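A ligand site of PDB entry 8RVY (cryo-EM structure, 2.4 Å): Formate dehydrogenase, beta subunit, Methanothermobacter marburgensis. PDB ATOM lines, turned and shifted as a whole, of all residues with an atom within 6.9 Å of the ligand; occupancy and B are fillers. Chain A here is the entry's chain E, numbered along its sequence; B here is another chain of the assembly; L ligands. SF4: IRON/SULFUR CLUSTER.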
ATOM      1  N   TRP A 277      18.014  15.657  15.870  1.00  0.00           N
ATOM      2  CA  TRP A 277      16.811  16.334  15.386  1.00  0.00           C
ATOM      3  C   TRP A 277      16.239  15.668  14.154  1.00  0.00           C
ATOM      4  O   TRP A 277      15.050  15.828  13.882  1.00  0.00           O
ATOM      5  CB  TRP A 277      17.108  17.810  15.090  1.00  0.00           C
ATOM      6  CG  TRP A 277      17.509  18.630  16.292  1.00  0.00           C
ATOM      7  CD1 TRP A 277      18.552  19.508  16.357  1.00  0.00           C
ATOM      8  CD2 TRP A 277      16.888  18.651  17.581  1.00  0.00           C
ATOM      9  NE1 TRP A 277      18.619  20.071  17.598  1.00  0.00           N
ATOM     10  CE2 TRP A 277      17.607  19.564  18.373  1.00  0.00           C
ATOM     11  CE3 TRP A 277      15.791  17.992  18.148  1.00  0.00           C
ATOM     12  CZ2 TRP A 277      17.267  19.832  19.696  1.00  0.00           C
ATOM     13  CZ3 TRP A 277      15.458  18.253  19.454  1.00  0.00           C
ATOM     14  CH2 TRP A 277      16.191  19.174  20.213  1.00  0.00           C
ATOM     15  N   ARG A 279      15.613  12.678  14.007  1.00  0.00           N
ATOM     16  CA  ARG A 279      14.785  11.592  14.500  1.00  0.00           C
ATOM     17  C   ARG A 279      13.382  12.031  14.905  1.00  0.00           C
ATOM     18  O   ARG A 279      12.465  11.197  14.900  1.00  0.00           O
ATOM     19  CB  ARG A 279      15.446  10.941  15.714  1.00  0.00           C
ATOM     20  CG  ARG A 279      16.249   9.709  15.377  1.00  0.00           C
ATOM     21  CD  ARG A 279      17.574   9.684  16.118  1.00  0.00           C
ATOM     22  NE  ARG A 279      17.408   9.300  17.508  1.00  0.00           N
ATOM     23  CZ  ARG A 279      18.350   8.715  18.249  1.00  0.00           C
ATOM     24  NH1 ARG A 279      19.535   8.435  17.745  1.00  0.00           N
ATOM     25  NH2 ARG A 279      18.086   8.420  19.515  1.00  0.00           N
ATOM     26  N   CYS A 280      13.189  13.313  15.216  1.00  0.00           N
ATOM     27  CA  CYS A 280      11.942  13.749  15.840  1.00  0.00           C
ATOM     28  C   CYS A 280      10.735  13.370  14.998  1.00  0.00           C
ATOM     29  O   CYS A 280      10.718  13.572  13.775  1.00  0.00           O
ATOM     30  CB  CYS A 280      11.990  15.259  16.049  1.00  0.00           C
ATOM     31  SG  CYS A 280      10.532  15.961  16.836  1.00  0.00           S
ATOM     32  N   ILE A 281       9.709  12.826  15.654  1.00  0.00           N
ATOM     33  CA  ILE A 281       8.479  12.405  14.992  1.00  0.00           C
ATOM     34  C   ILE A 281       7.340  13.371  15.243  1.00  0.00           C
ATOM     35  O   ILE A 281       6.199  13.079  14.881  1.00  0.00           O
ATOM     36  CB  ILE A 281       8.089  10.981  15.401  1.00  0.00           C
ATOM     37  CG1 ILE A 281       7.987  10.855  16.925  1.00  0.00           C
ATOM     38  CG2 ILE A 281       9.074   9.969  14.847  1.00  0.00           C
ATOM     39  CD1 ILE A 281       6.934   9.898  17.386  1.00  0.00           C
ATOM     40  N   ASN A 282       7.611  14.517  15.866  1.00  0.00           N
ATOM     41  CA  ASN A 282       6.615  15.579  15.990  1.00  0.00           C
ATOM     42  C   ASN A 282       5.410  15.127  16.811  1.00  0.00           C
ATOM     43  O   ASN A 282       4.272  15.517  16.550  1.00  0.00           O
ATOM     44  CB  ASN A 282       6.181  16.065  14.603  1.00  0.00           C
ATOM     45  CG  ASN A 282       5.708  17.508  14.603  1.00  0.00           C
ATOM     46  OD1 ASN A 282       6.083  18.292  15.461  1.00  0.00           O
ATOM     47  ND2 ASN A 282       4.879  17.849  13.626  1.00  0.00           N
ATOM     48  N   CYS A 283       5.661  14.283  17.809  1.00  0.00           N
ATOM     49  CA  CYS A 283       4.583  13.721  18.612  1.00  0.00           C
ATOM     50  C   CYS A 283       4.138  14.650  19.732  1.00  0.00           C
ATOM     51  O   CYS A 283       3.038  14.467  20.259  1.00  0.00           O
ATOM     52  CB  CYS A 283       5.019  12.384  19.203  1.00  0.00           C
ATOM     53  SG  CYS A 283       6.302  12.500  20.472  1.00  0.00           S
ATOM     54  N   PHE A 284       4.967  15.624  20.118  1.00  0.00           N
ATOM     55  CA  PHE A 284       4.669  16.618  21.148  1.00  0.00           C
ATOM     56  C   PHE A 284       4.638  16.026  22.551  1.00  0.00           C
ATOM     57  O   PHE A 284       4.056  16.626  23.453  1.00  0.00           O
ATOM     58  CB  PHE A 284       3.347  17.337  20.863  1.00  0.00           C
ATOM     59  CG  PHE A 284       3.426  18.341  19.757  1.00  0.00           C
ATOM     60  CD1 PHE A 284       3.882  19.621  20.001  1.00  0.00           C
ATOM     61  CD2 PHE A 284       3.064  18.008  18.471  1.00  0.00           C
ATOM     62  CE1 PHE A 284       3.965  20.547  18.985  1.00  0.00           C
ATOM     63  CE2 PHE A 284       3.136  18.925  17.454  1.00  0.00           C
ATOM     64  CZ  PHE A 284       3.596  20.200  17.714  1.00  0.00           C
ATOM     65  N   ALA A 285       5.249  14.867  22.764  1.00  0.00           N
ATOM     66  CA  ALA A 285       5.287  14.289  24.110  1.00  0.00           C
ATOM     67  C   ALA A 285       6.103  15.153  25.055  1.00  0.00           C
ATOM     68  O   ALA A 285       5.769  15.288  26.237  1.00  0.00           O
ATOM     69  CB  ALA A 285       5.838  12.868  24.053  1.00  0.00           C
ATOM     70  N   CYS A 286       7.196  15.748  24.547  1.00  0.00           N
ATOM     71  CA  CYS A 286       8.000  16.647  25.369  1.00  0.00           C
ATOM     72  C   CYS A 286       7.187  17.848  25.830  1.00  0.00           C
ATOM     73  O   CYS A 286       7.242  18.238  26.995  1.00  0.00           O
ATOM     74  CB  CYS A 286       9.224  17.097  24.581  1.00  0.00           C
ATOM     75  SG  CYS A 286       8.838  17.661  22.906  1.00  0.00           S
ATOM     76  N   ARG A 287       6.432  18.441  24.911  1.00  0.00           N
ATOM     77  CA  ARG A 287       5.585  19.570  25.269  1.00  0.00           C
ATOM     78  C   ARG A 287       4.517  19.170  26.278  1.00  0.00           C
ATOM     79  O   ARG A 287       4.265  19.894  27.250  1.00  0.00           O
ATOM     80  CB  ARG A 287       4.937  20.137  24.001  1.00  0.00           C
ATOM     81  CG  ARG A 287       4.469  21.587  24.117  1.00  0.00           C
ATOM     82  CD  ARG A 287       3.056  21.735  24.668  1.00  0.00           C
ATOM     83  NE  ARG A 287       2.149  20.670  24.261  1.00  0.00           N
ATOM     84  CZ  ARG A 287       1.704  20.492  23.017  1.00  0.00           C
ATOM     85  NH1 ARG A 287       2.093  21.262  22.021  1.00  0.00           N
ATOM     86  NH2 ARG A 287       0.858  19.502  22.770  1.00  0.00           N
ATOM     87  N   PRO A 313      10.430  17.703  12.116  1.00  0.00           N
ATOM     88  CA  PRO A 313      10.248  19.163  12.072  1.00  0.00           C
ATOM     89  C   PRO A 313      11.569  19.884  11.948  1.00  0.00           C
ATOM     90  O   PRO A 313      12.634  19.366  12.274  1.00  0.00           O
ATOM     91  CB  PRO A 313       9.564  19.487  13.411  1.00  0.00           C
ATOM     92  CG  PRO A 313       9.228  18.188  14.025  1.00  0.00           C
ATOM     93  CD  PRO A 313      10.118  17.157  13.438  1.00  0.00           C
ATOM     94  N   PHE A 318      10.158  24.411  16.055  1.00  0.00           N
ATOM     95  CA  PHE A 318       9.642  23.622  17.166  1.00  0.00           C
ATOM     96  C   PHE A 318      10.396  23.939  18.452  1.00  0.00           C
ATOM     97  O   PHE A 318       9.863  24.555  19.392  1.00  0.00           O
ATOM     98  CB  PHE A 318       9.738  22.132  16.826  1.00  0.00           C
ATOM     99  CG  PHE A 318       8.962  21.229  17.731  1.00  0.00           C
ATOM    100  CD1 PHE A 318       9.438  20.911  19.000  1.00  0.00           C
ATOM    101  CD2 PHE A 318       7.773  20.674  17.326  1.00  0.00           C
ATOM    102  CE1 PHE A 318       8.728  20.069  19.829  1.00  0.00           C
ATOM    103  CE2 PHE A 318       7.054  19.832  18.151  1.00  0.00           C
ATOM    104  CZ  PHE A 318       7.534  19.542  19.410  1.00  0.00           C
ATOM    105  N   GLN A 319      11.685  23.582  18.464  1.00  0.00           N
ATOM    106  CA  GLN A 319      12.464  23.641  19.690  1.00  0.00           C
ATOM    107  C   GLN A 319      12.829  25.067  20.045  1.00  0.00           C
ATOM    108  O   GLN A 319      12.712  25.461  21.205  1.00  0.00           O
ATOM    109  CB  GLN A 319      13.721  22.776  19.542  1.00  0.00           C
ATOM    110  CG  GLN A 319      13.457  21.332  19.179  1.00  0.00           C
ATOM    111  CD  GLN A 319      12.747  20.572  20.288  1.00  0.00           C
ATOM    112  OE1 GLN A 319      12.586  21.073  21.399  1.00  0.00           O
ATOM    113  NE2 GLN A 319      12.308  19.363  19.978  1.00  0.00           N
ATOM    114  N   ARG A 322       9.720  26.805  21.415  1.00  0.00           N
ATOM    115  CA  ARG A 322       9.430  26.434  22.793  1.00  0.00           C
ATOM    116  C   ARG A 322      10.468  27.014  23.750  1.00  0.00           C
ATOM    117  O   ARG A 322      10.134  27.388  24.883  1.00  0.00           O
ATOM    118  CB  ARG A 322       9.351  24.917  22.933  1.00  0.00           C
ATOM    119  CG  ARG A 322       8.619  24.448  24.171  1.00  0.00           C
ATOM    120  CD  ARG A 322       8.212  22.991  24.089  1.00  0.00           C
ATOM    121  NE  ARG A 322       9.250  22.095  24.577  1.00  0.00           N
ATOM    122  CZ  ARG A 322       9.561  21.909  25.850  1.00  0.00           C
ATOM    123  NH1 ARG A 322       8.928  22.549  26.819  1.00  0.00           N
ATOM    124  NH2 ARG A 322      10.527  21.054  26.175  1.00  0.00           N
ATOM    125  N   CYS A 336      10.536  15.963  29.811  1.00  0.00           N
ATOM    126  CA  CYS A 336      10.545  15.997  28.352  1.00  0.00           C
ATOM    127  C   CYS A 336      11.471  14.935  27.782  1.00  0.00           C
ATOM    128  O   CYS A 336      11.119  14.219  26.849  1.00  0.00           O
ATOM    129  CB  CYS A 336      10.967  17.381  27.869  1.00  0.00           C
ATOM    130  SG  CYS A 336      12.575  17.934  28.489  1.00  0.00           S
ATOM    131  N   VAL A 339       9.990  11.286  28.374  1.00  0.00           N
ATOM    132  CA  VAL A 339       8.886  10.777  27.570  1.00  0.00           C
ATOM    133  C   VAL A 339       9.194  10.743  26.071  1.00  0.00           C
ATOM    134  O   VAL A 339       8.352  10.278  25.292  1.00  0.00           O
ATOM    135  CB  VAL A 339       7.614  11.618  27.802  1.00  0.00           C
ATOM    136  CG1 VAL A 339       7.194  11.558  29.256  1.00  0.00           C
ATOM    137  CG2 VAL A 339       7.813  13.047  27.355  1.00  0.00           C
ATOM    138  N   CYS A 340      10.361  11.215  25.643  1.00  0.00           N
ATOM    139  CA  CYS A 340      10.617  11.319  24.217  1.00  0.00           C
ATOM    140  C   CYS A 340      10.706   9.927  23.592  1.00  0.00           C
ATOM    141  O   CYS A 340      11.596   9.153  23.968  1.00  0.00           O
ATOM    142  CB  CYS A 340      11.918  12.084  23.962  1.00  0.00           C
ATOM    143  SG  CYS A 340      12.302  12.350  22.214  1.00  0.00           S
ATOM    144  N   PRO A 341       9.840   9.578  22.640  1.00  0.00           N
ATOM    145  CA  PRO A 341       9.934   8.243  22.029  1.00  0.00           C
ATOM    146  C   PRO A 341      11.185   8.046  21.196  1.00  0.00           C
ATOM    147  O   PRO A 341      11.480   6.900  20.828  1.00  0.00           O
ATOM    148  CB  PRO A 341       8.679   8.168  21.150  1.00  0.00           C
ATOM    149  CG  PRO A 341       7.800   9.274  21.585  1.00  0.00           C
ATOM    150  CD  PRO A 341       8.684  10.333  22.123  1.00  0.00           C
ATOM    151  N   MET A 342      11.922   9.100  20.886  1.00  0.00           N
ATOM    152  CA  MET A 342      13.094   9.005  20.037  1.00  0.00           C
ATOM    153  C   MET A 342      14.405   9.111  20.812  1.00  0.00           C
ATOM    154  O   MET A 342      15.469   9.064  20.187  1.00  0.00           O
ATOM    155  CB  MET A 342      13.039  10.103  18.963  1.00  0.00           C
ATOM    156  CG  MET A 342      12.180   9.761  17.745  1.00  0.00           C
ATOM    157  SD  MET A 342      12.429   8.105  17.073  1.00  0.00           S
ATOM    158  CE  MET A 342      10.808   7.383  17.313  1.00  0.00           C
ATOM    159  N   ASP A 343      14.346   9.242  22.136  1.00  0.00           N
ATOM    160  CA  ASP A 343      15.548   9.307  22.962  1.00  0.00           C
ATOM    161  C   ASP A 343      16.436  10.496  22.582  1.00  0.00           C
ATOM    162  O   ASP A 343      17.646  10.363  22.401  1.00  0.00           O
ATOM    163  CB  ASP A 343      16.334   7.996  22.893  1.00  0.00           C
ATOM    164  CG  ASP A 343      15.567   6.825  23.446  1.00  0.00           C
ATOM    165  OD1 ASP A 343      14.828   7.018  24.430  1.00  0.00           O
ATOM    166  OD2 ASP A 343      15.690   5.719  22.895  1.00  0.00           O
ATOM    167  N   ILE A 344      15.810  11.654  22.456  1.00  0.00           N
ATOM    168  CA  ILE A 344      16.522  12.903  22.208  1.00  0.00           C
ATOM    169  C   ILE A 344      16.848  13.537  23.555  1.00  0.00           C
ATOM    170  O   ILE A 344      15.972  13.606  24.426  1.00  0.00           O
ATOM    171  CB  ILE A 344      15.715  13.852  21.311  1.00  0.00           C
ATOM    172  CG1 ILE A 344      15.591  13.272  19.900  1.00  0.00           C
ATOM    173  CG2 ILE A 344      16.353  15.220  21.261  1.00  0.00           C
ATOM    174  CD1 ILE A 344      14.429  13.822  19.114  1.00  0.00           C
ATOM    175  N   ILE A 346      16.614  16.325  25.139  1.00  0.00           N
ATOM    176  CA  ILE A 346      16.026  17.675  25.128  1.00  0.00           C
ATOM    177  C   ILE A 346      16.449  18.457  26.354  1.00  0.00           C
ATOM    178  O   ILE A 346      16.808  19.652  26.265  1.00  0.00           O
ATOM    179  CB  ILE A 346      14.484  17.566  25.042  1.00  0.00           C
ATOM    180  CG1 ILE A 346      14.027  16.666  23.894  1.00  0.00           C
ATOM    181  CG2 ILE A 346      13.872  18.935  24.884  1.00  0.00           C
ATOM    182  CD1 ILE A 346      12.729  15.971  24.169  1.00  0.00           C
ATOM    183  N   THR B  42       5.277   7.530  24.588  1.00  0.00           N
ATOM    184  CA  THR B  42       4.158   7.282  23.696  1.00  0.00           C
ATOM    185  C   THR B  42       4.202   8.276  22.545  1.00  0.00           C
ATOM    186  O   THR B  42       4.739   9.378  22.674  1.00  0.00           O
ATOM    187  CB  THR B  42       2.807   7.389  24.406  1.00  0.00           C
ATOM    188  OG1 THR B  42       2.717   8.650  25.083  1.00  0.00           O
ATOM    189  CG2 THR B  42       2.622   6.280  25.404  1.00  0.00           C
ATOM    190  N   ARG B  47      -1.262   9.180  23.559  1.00  0.00           N
ATOM    191  CA  ARG B  47      -1.657  10.171  24.537  1.00  0.00           C
ATOM    192  C   ARG B  47      -3.061  10.709  24.312  1.00  0.00           C
ATOM    193  O   ARG B  47      -3.566  11.464  25.139  1.00  0.00           O
ATOM    194  CB  ARG B  47      -0.661  11.333  24.538  1.00  0.00           C
ATOM    195  CG  ARG B  47       0.409  11.203  25.616  1.00  0.00           C
ATOM    196  CD  ARG B  47       1.595  12.109  25.349  1.00  0.00           C
ATOM    197  NE  ARG B  47       2.312  11.737  24.136  1.00  0.00           N
ATOM    198  CZ  ARG B  47       2.388  12.465  23.034  1.00  0.00           C
ATOM    199  NH1 ARG B  47       1.764  13.630  22.929  1.00  0.00           N
ATOM    200  NH2 ARG B  47       3.094  12.015  21.998  1.00  0.00           N
HETATM  201 FE1  SF4 L   1      10.815  13.729  21.156  1.00  0.00          FE
HETATM  202 FE2  SF4 L   1       9.339  16.019  21.398  1.00  0.00          FE
HETATM  203 FE3  SF4 L   1       8.206  13.758  20.338  1.00  0.00          FE
HETATM  204 FE4  SF4 L   1      10.098  15.145  18.920  1.00  0.00          FE
HETATM  205  S1  SF4 L   1       8.029  15.880  19.535  1.00  0.00           S
HETATM  206  S2  SF4 L   1       9.983  12.885  19.212  1.00  0.00           S
HETATM  207  S3  SF4 L   1      11.461  15.848  20.616  1.00  0.00           S
HETATM  208  S4  SF4 L   1       8.967  14.035  22.466  1.00  0.00           S
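Asn 282 touches the ligand (CA to S1, 3.8 Å).
Ala 285 touches the ligand (CB to S4, 3.7 Å).
Phe 318 touches the ligand (CZ to S1, 3.7 Å).
CD of Pro 341 touches S4 of the ligand (3.7 Å).
Ile 344 touches the ligand.
CD1 of Ile 346 touches S3 of the ligand, 3.8 Å away.
Hydrophobic or aromatic side chains that line the ligand: Ile 281, Ala 285, Phe 318, Pro 341, Ile 344 and Ile 346.
Of the 24 residues printed, 13 come within 4 Å of the ligand.
The nearest printed residue that does not touch the ligand is Met 342 (4.1 Å).
An iron atom (FE4) of the ligand is bound by the side-chain sulfur (SG) of Cys 280, 2.3 Å away.
The side-chain sulfur of Cys 340 is bound to an iron atom (FE1) of the ligand, at 2.3 Å.
The backbone NH (N) of Phe 284 lies close to a sulfur (S1) of the ligand.
The backbone NH (N) of Ile 281 lies close to a sulfur (S2) of the ligand, 3.6 Å away.
A sulfur (S1) of the ligand sits close to the backbone NH (N) of Cys 283 (3.3 Å).
FE3 of the ligand is bound by SG of Cys 283 (2.3 Å).
The backbone NH (N) of Cys 286 sits close to a sulfur (S4) of the ligand, 3.2 Å away.
The side-chain sulfur (SG) of Cys 286 binds an iron atom (FE2) of the ligand, at 2.3 Å.
The side-chain amide nitrogen of Gln 319 sits close to a sulfur (S3) of the ligand.
N of Ala 285 sits close to SG of Cys 283, 3.5 Å away.
The side-chain sulfur of Cys 340 lies close to the backbone NH of Asp 343 (3.7 Å).
The backbone NH of Met 342 sits close to the side-chain sulfur of Cys 340, at 3.5 Å.
The guanidinium group of Arg 47 of chain B lies within hydrogen-bond range of the backbone carbonyl oxygen of Cys 283 (3.0 Å).
The side-chain sulfur (SG) of Cys 280 lies close to the backbone NH (N) of Asn 282 (3.4 Å).
The backbone NH (N) of Ile 344 sits close to the side-chain sulfur (SG) of Cys 340, at 3.6 Å.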
